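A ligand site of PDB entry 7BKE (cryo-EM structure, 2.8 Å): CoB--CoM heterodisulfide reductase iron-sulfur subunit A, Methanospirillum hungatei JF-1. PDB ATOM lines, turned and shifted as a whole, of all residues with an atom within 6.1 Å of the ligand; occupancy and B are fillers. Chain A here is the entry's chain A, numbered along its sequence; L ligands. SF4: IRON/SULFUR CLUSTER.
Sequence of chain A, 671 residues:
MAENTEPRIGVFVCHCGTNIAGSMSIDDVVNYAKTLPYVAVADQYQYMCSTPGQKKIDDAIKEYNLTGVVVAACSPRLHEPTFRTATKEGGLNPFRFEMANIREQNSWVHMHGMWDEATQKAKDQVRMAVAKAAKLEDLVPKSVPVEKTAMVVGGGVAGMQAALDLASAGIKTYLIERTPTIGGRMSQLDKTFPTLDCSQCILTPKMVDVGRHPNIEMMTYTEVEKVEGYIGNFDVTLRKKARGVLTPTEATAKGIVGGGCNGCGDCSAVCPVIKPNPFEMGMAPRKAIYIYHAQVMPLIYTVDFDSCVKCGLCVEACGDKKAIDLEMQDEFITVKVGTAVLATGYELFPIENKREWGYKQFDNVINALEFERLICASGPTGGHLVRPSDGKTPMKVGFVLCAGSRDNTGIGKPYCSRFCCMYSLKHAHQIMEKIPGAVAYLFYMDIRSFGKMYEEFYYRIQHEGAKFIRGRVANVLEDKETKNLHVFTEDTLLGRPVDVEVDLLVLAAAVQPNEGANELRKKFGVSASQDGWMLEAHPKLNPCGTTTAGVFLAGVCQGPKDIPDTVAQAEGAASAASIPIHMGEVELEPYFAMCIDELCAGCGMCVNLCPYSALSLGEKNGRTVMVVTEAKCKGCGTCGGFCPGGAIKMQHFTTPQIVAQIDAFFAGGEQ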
ATOM      1  N   LEU A 401       8.603   8.120  -6.158  1.00  0.00           N
ATOM      2  CA  LEU A 401       8.447   6.977  -7.078  1.00  0.00           C
ATOM      3  C   LEU A 401       8.693   7.453  -8.495  1.00  0.00           C
ATOM      4  O   LEU A 401       8.574   8.657  -8.719  1.00  0.00           O
ATOM      5  CB  LEU A 401       7.030   6.427  -6.923  1.00  0.00           C
ATOM      6  CG  LEU A 401       6.824   5.371  -5.839  1.00  0.00           C
ATOM      7  CD1 LEU A 401       6.833   6.003  -4.456  1.00  0.00           C
ATOM      8  CD2 LEU A 401       5.522   4.634  -6.061  1.00  0.00           C
ATOM      9  N   CYS A 402       9.167   6.580  -9.368  1.00  0.00           N
ATOM     10  CA  CYS A 402       9.348   6.883 -10.806  1.00  0.00           C
ATOM     11  C   CYS A 402      10.592   7.757 -10.962  1.00  0.00           C
ATOM     12  O   CYS A 402      10.669   8.459 -11.936  1.00  0.00           O
ATOM     13  CB  CYS A 402       8.091   7.446 -11.457  1.00  0.00           C
ATOM     14  SG  CYS A 402       6.825   6.247 -11.930  1.00  0.00           S
ATOM     15  N   ALA A 403      11.508   7.693 -10.018  1.00  0.00           N
ATOM     16  CA  ALA A 403      12.682   8.571 -10.025  1.00  0.00           C
ATOM     17  C   ALA A 403      13.594   8.175 -11.166  1.00  0.00           C
ATOM     18  O   ALA A 403      14.384   7.234 -11.048  1.00  0.00           O
ATOM     19  CB  ALA A 403      13.401   8.518  -8.697  1.00  0.00           C
ATOM     20  N   SER A 405      12.377   7.355 -14.240  1.00  0.00           N
ATOM     21  CA  SER A 405      11.706   6.302 -15.036  1.00  0.00           C
ATOM     22  C   SER A 405      10.534   6.877 -15.829  1.00  0.00           C
ATOM     23  O   SER A 405      10.065   7.922 -15.473  1.00  0.00           O
ATOM     24  CB  SER A 405      11.330   5.161 -14.162  1.00  0.00           C
ATOM     25  OG  SER A 405      12.132   5.112 -13.000  1.00  0.00           O
ATOM     26  N   ARG A 406      10.093   6.171 -16.859  1.00  0.00           N
ATOM     27  CA  ARG A 406       8.975   6.628 -17.717  1.00  0.00           C
ATOM     28  C   ARG A 406       9.339   8.075 -18.066  1.00  0.00           C
ATOM     29  O   ARG A 406       8.423   8.891 -18.087  1.00  0.00           O
ATOM     30  CB  ARG A 406       7.684   6.355 -16.955  1.00  0.00           C
ATOM     31  CG  ARG A 406       7.680   5.052 -16.179  1.00  0.00           C
ATOM     32  CD  ARG A 406       6.440   4.943 -15.325  1.00  0.00           C
ATOM     33  NE  ARG A 406       5.298   5.483 -16.040  1.00  0.00           N
ATOM     34  CZ  ARG A 406       4.170   5.868 -15.471  1.00  0.00           C
ATOM     35  NH1 ARG A 406       4.019   5.752 -14.167  1.00  0.00           N
ATOM     36  NH2 ARG A 406       3.188   6.331 -16.206  1.00  0.00           N
ATOM     37  N   TYR A 415      11.403   3.544 -19.599  1.00  0.00           N
ATOM     38  CA  TYR A 415      10.623   2.373 -19.263  1.00  0.00           C
ATOM     39  C   TYR A 415      10.272   2.362 -17.781  1.00  0.00           C
ATOM     40  O   TYR A 415      10.759   3.171 -16.988  1.00  0.00           O
ATOM     41  CB  TYR A 415      11.371   1.083 -19.646  1.00  0.00           C
ATOM     42  CG  TYR A 415      12.797   1.015 -19.148  1.00  0.00           C
ATOM     43  CD1 TYR A 415      13.850   1.248 -20.004  1.00  0.00           C
ATOM     44  CD2 TYR A 415      13.082   0.712 -17.837  1.00  0.00           C
ATOM     45  CE1 TYR A 415      15.144   1.183 -19.563  1.00  0.00           C
ATOM     46  CE2 TYR A 415      14.370   0.653 -17.385  1.00  0.00           C
ATOM     47  CZ  TYR A 415      15.394   0.889 -18.264  1.00  0.00           C
ATOM     48  OH  TYR A 415      16.686   0.821 -17.814  1.00  0.00           O
ATOM     49  N   CYS A 416       9.405   1.445 -17.401  1.00  0.00           N
ATOM     50  CA  CYS A 416       9.051   1.243 -15.979  1.00  0.00           C
ATOM     51  C   CYS A 416      10.032   0.201 -15.456  1.00  0.00           C
ATOM     52  O   CYS A 416      10.261  -0.767 -16.156  1.00  0.00           O
ATOM     53  CB  CYS A 416       7.611   0.764 -15.902  1.00  0.00           C
ATOM     54  SG  CYS A 416       7.048   0.207 -14.276  1.00  0.00           S
ATOM     55  N   SER A 417      10.525   0.380 -14.254  1.00  0.00           N
ATOM     56  CA  SER A 417      11.457  -0.582 -13.623  1.00  0.00           C
ATOM     57  C   SER A 417      10.696  -1.715 -12.921  1.00  0.00           C
ATOM     58  O   SER A 417      11.350  -2.425 -12.188  1.00  0.00           O
ATOM     59  CB  SER A 417      12.497   0.068 -12.801  1.00  0.00           C
ATOM     60  OG  SER A 417      13.449   0.699 -13.629  1.00  0.00           O
ATOM     61  N   ARG A 418       9.373  -1.783 -13.046  1.00  0.00           N
ATOM     62  CA  ARG A 418       8.549  -2.941 -12.598  1.00  0.00           C
ATOM     63  C   ARG A 418       8.363  -3.092 -11.089  1.00  0.00           C
ATOM     64  O   ARG A 418       7.232  -3.228 -10.687  1.00  0.00           O
ATOM     65  CB  ARG A 418       8.980  -4.233 -13.283  1.00  0.00           C
ATOM     66  CG  ARG A 418       7.926  -5.316 -13.314  1.00  0.00           C
ATOM     67  CD  ARG A 418       8.282  -6.280 -14.412  1.00  0.00           C
ATOM     68  NE  ARG A 418       7.636  -7.570 -14.236  1.00  0.00           N
ATOM     69  CZ  ARG A 418       7.288  -8.349 -15.242  1.00  0.00           C
ATOM     70  NH1 ARG A 418       7.545  -7.969 -16.485  1.00  0.00           N
ATOM     71  NH2 ARG A 418       6.692  -9.501 -15.013  1.00  0.00           N
ATOM     72  N   PHE A 419       9.421  -3.091 -10.297  1.00  0.00           N
ATOM     73  CA  PHE A 419       9.307  -3.397  -8.851  1.00  0.00           C
ATOM     74  C   PHE A 419       9.392  -2.201  -7.916  1.00  0.00           C
ATOM     75  O   PHE A 419       9.279  -2.424  -6.718  1.00  0.00           O
ATOM     76  CB  PHE A 419      10.359  -4.440  -8.434  1.00  0.00           C
ATOM     77  CG  PHE A 419      11.718  -4.339  -9.076  1.00  0.00           C
ATOM     78  CD1 PHE A 419      12.129  -5.263 -10.012  1.00  0.00           C
ATOM     79  CD2 PHE A 419      12.617  -3.355  -8.686  1.00  0.00           C
ATOM     80  CE1 PHE A 419      13.393  -5.188 -10.580  1.00  0.00           C
ATOM     81  CE2 PHE A 419      13.880  -3.281  -9.254  1.00  0.00           C
ATOM     82  CZ  PHE A 419      14.269  -4.204 -10.192  1.00  0.00           C
ATOM     83  N   CYS A 420       9.639  -1.013  -8.431  1.00  0.00           N
ATOM     84  CA  CYS A 420       9.872   0.187  -7.559  1.00  0.00           C
ATOM     85  C   CYS A 420       8.607   0.680  -6.845  1.00  0.00           C
ATOM     86  O   CYS A 420       8.755   1.274  -5.787  1.00  0.00           O
ATOM     87  CB  CYS A 420      10.663   1.299  -8.252  1.00  0.00           C
ATOM     88  SG  CYS A 420      10.821   1.118 -10.028  1.00  0.00           S
ATOM     89  N   CYS A 421       7.419   0.379  -7.346  1.00  0.00           N
ATOM     90  CA  CYS A 421       6.170   0.771  -6.655  1.00  0.00           C
ATOM     91  C   CYS A 421       6.013  -0.187  -5.487  1.00  0.00           C
ATOM     92  O   CYS A 421       5.687   0.256  -4.415  1.00  0.00           O
ATOM     93  CB  CYS A 421       4.920   0.660  -7.521  1.00  0.00           C
ATOM     94  SG  CYS A 421       4.587   2.002  -8.684  1.00  0.00           S
ATOM     95  N   MET A 422       6.341  -1.452  -5.699  1.00  0.00           N
ATOM     96  CA  MET A 422       6.149  -2.476  -4.688  1.00  0.00           C
ATOM     97  C   MET A 422       7.157  -2.341  -3.555  1.00  0.00           C
ATOM     98  O   MET A 422       6.789  -2.422  -2.385  1.00  0.00           O
ATOM     99  CB  MET A 422       6.250  -3.856  -5.323  1.00  0.00           C
ATOM    100  CG  MET A 422       5.022  -4.264  -6.117  1.00  0.00           C
ATOM    101  SD  MET A 422       3.437  -4.009  -5.318  1.00  0.00           S
ATOM    102  CE  MET A 422       3.645  -4.979  -3.835  1.00  0.00           C
ATOM    103  N   SER A 424       8.687   0.383  -2.695  1.00  0.00           N
ATOM    104  CA  SER A 424       8.397   1.610  -1.968  1.00  0.00           C
ATOM    105  C   SER A 424       7.257   1.397  -0.972  1.00  0.00           C
ATOM    106  O   SER A 424       7.300   1.917   0.146  1.00  0.00           O
ATOM    107  CB  SER A 424       8.061   2.741  -2.925  1.00  0.00           C
ATOM    108  OG  SER A 424       9.118   2.944  -3.841  1.00  0.00           O
ATOM    109  N   MET A 445       2.763   8.255  -9.246  1.00  0.00           N
ATOM    110  CA  MET A 445       2.176   8.638 -10.555  1.00  0.00           C
ATOM    111  C   MET A 445       1.805   7.329 -11.212  1.00  0.00           C
ATOM    112  O   MET A 445       2.602   6.910 -12.061  1.00  0.00           O
ATOM    113  CB  MET A 445       3.306   9.281 -11.357  1.00  0.00           C
ATOM    114  CG  MET A 445       2.981   9.749 -12.745  1.00  0.00           C
ATOM    115  SD  MET A 445       4.532  10.354 -13.420  1.00  0.00           S
ATOM    116  CE  MET A 445       5.363   8.855 -13.910  1.00  0.00           C
ATOM    117  N   ASP A 446       0.766   6.643 -10.763  1.00  0.00           N
ATOM    118  CA  ASP A 446       0.409   5.267 -11.217  1.00  0.00           C
ATOM    119  C   ASP A 446       1.007   4.203 -10.312  1.00  0.00           C
ATOM    120  O   ASP A 446       2.071   3.730 -10.642  1.00  0.00           O
ATOM    121  CB  ASP A 446       0.615   4.914 -12.697  1.00  0.00           C
ATOM    122  CG  ASP A 446      -0.207   5.718 -13.688  1.00  0.00           C
ATOM    123  OD1 ASP A 446      -1.417   5.454 -13.797  1.00  0.00           O
ATOM    124  OD2 ASP A 446       0.383   6.562 -14.362  1.00  0.00           O
ATOM    125  N   ILE A 447       0.393   3.932  -9.170  1.00  0.00           N
ATOM    126  CA  ILE A 447       0.767   2.769  -8.362  1.00  0.00           C
ATOM    127  C   ILE A 447       0.561   1.502  -9.174  1.00  0.00           C
ATOM    128  O   ILE A 447      -0.520   1.263  -9.728  1.00  0.00           O
ATOM    129  CB  ILE A 447      -0.069   2.721  -7.066  1.00  0.00           C
ATOM    130  CG1 ILE A 447       0.239   3.905  -6.158  1.00  0.00           C
ATOM    131  CG2 ILE A 447       0.211   1.425  -6.324  1.00  0.00           C
ATOM    132  CD1 ILE A 447       1.540   3.801  -5.445  1.00  0.00           C
ATOM    133  N   ARG A 448       1.610   0.670  -9.265  1.00  0.00           N
ATOM    134  CA  ARG A 448       1.624  -0.519 -10.164  1.00  0.00           C
ATOM    135  C   ARG A 448       1.788  -1.797  -9.340  1.00  0.00           C
ATOM    136  O   ARG A 448       2.887  -2.303  -9.246  1.00  0.00           O
ATOM    137  CB  ARG A 448       2.657  -0.320 -11.292  1.00  0.00           C
ATOM    138  CG  ARG A 448       2.183   0.616 -12.391  1.00  0.00           C
ATOM    139  CD  ARG A 448       3.180   0.820 -13.521  1.00  0.00           C
ATOM    140  NE  ARG A 448       2.594   1.732 -14.485  1.00  0.00           N
ATOM    141  CZ  ARG A 448       3.180   2.152 -15.591  1.00  0.00           C
ATOM    142  NH1 ARG A 448       2.549   2.978 -16.396  1.00  0.00           N
ATOM    143  NH2 ARG A 448       4.409   1.759 -15.869  1.00  0.00           N
ATOM    144  N   ALA A 508      13.109   6.194  -5.443  1.00  0.00           N
ATOM    145  CA  ALA A 508      12.918   4.883  -6.057  1.00  0.00           C
ATOM    146  C   ALA A 508      13.476   4.947  -7.478  1.00  0.00           C
ATOM    147  O   ALA A 508      12.755   5.101  -8.467  1.00  0.00           O
ATOM    148  CB  ALA A 508      11.449   4.483  -6.047  1.00  0.00           C
HETATM  149 FE1  SF4 L   1       8.933   1.997 -10.615  1.00  0.00          FE
HETATM  150 FE2  SF4 L   1       7.454   4.158 -11.401  1.00  0.00          FE
HETATM  151 FE3  SF4 L   1       6.246   2.091 -10.134  1.00  0.00          FE
HETATM  152 FE4  SF4 L   1       7.201   1.772 -12.707  1.00  0.00          FE
HETATM  153  S1  SF4 L   1       5.516   3.149 -12.015  1.00  0.00           S
HETATM  154  S2  SF4 L   1       7.419   0.334 -10.938  1.00  0.00           S
HETATM  155  S3  SF4 L   1       9.045   3.052 -12.607  1.00  0.00           S
HETATM  156  S4  SF4 L   1       7.828   3.477  -9.271  1.00  0.00           S
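The backbone carbonyl oxygen of Asp 446 lies close to a sulfur (S1) of the ligand (3.8 Å).
CB of Leu 401 touches S4 of the ligand, 3.9 Å away.
CD of Arg 448 touches S1 of the ligand, at 3.6 Å.
Hydrophobic or aromatic side chains that line the ligand: Leu 401.
Of the 19 residues printed, 11 come within 4 Å of the ligand.
The nearest printed residue that does not touch the ligand is Phe 419 (4.02 Å).
The backbone NH of Cys 420 lies close to a sulfur (S2) of the ligand, 3.6 Å away.
An iron atom (FE1) of the ligand is bound by the side-chain sulfur (SG) of Cys 420 (2.2 Å).
The backbone NH (N) of Cys 421 sits close to a sulfur (S2) of the ligand (3.6 Å).
An iron atom (FE3) of the ligand is bound by the side-chain sulfur of Cys 421 (2.2 Å).
The side-chain sulfur (SG) of Cys 416 binds an iron atom (FE4) of the ligand (2.2 Å).
N of Cys 402 sits close to S4 of the ligand (3.4 Å).
The side-chain sulfur (SG) of Cys 402 is bound to an iron atom (FE2) of the ligand (2.2 Å).
The backbone NH (N) of Ser 417 sits close to a sulfur (S3) of the ligand (3.5 Å).
S3 of the ligand lies close to OG of Ser 405 (3.7 Å).
A sulfur (S2) of the ligand lies close to the backbone NH (N) of Arg 418 (3.6 Å).
The guanidinium group (NH1) of Arg 406 sits close to a sulfur (S1) of the ligand (3.7 Å).
The backbone carbonyl oxygen of Cys 420 sits at hydrogen-bond distance from the side-chain hydroxyl of Ser 424, at 2.6 Å.
SG of Cys 421 lies close to N of Arg 448, at 3.3 Å.
The side-chain sulfur (SG) of Cys 421 lies close to the backbone carbonyl oxygen (O) of Asp 446, at 3.6 Å.
The backbone NH of Arg 418 lies close to the side-chain sulfur of Cys 416, 3.3 Å away.
SG of Cys 416 sits close to NH2 of Arg 448, at 3.5 Å.
SG of Cys 402 lies close to NH1 of Arg 406 (3.6 Å).
The backbone NH of Arg 406 is in hydrogen-bond range of the backbone carbonyl oxygen of Tyr 415, 3.1 Å away.
The guanidinium group (NH1) of Arg 406 is in hydrogen-bond range of the backbone carbonyl oxygen (O) of Met 445.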
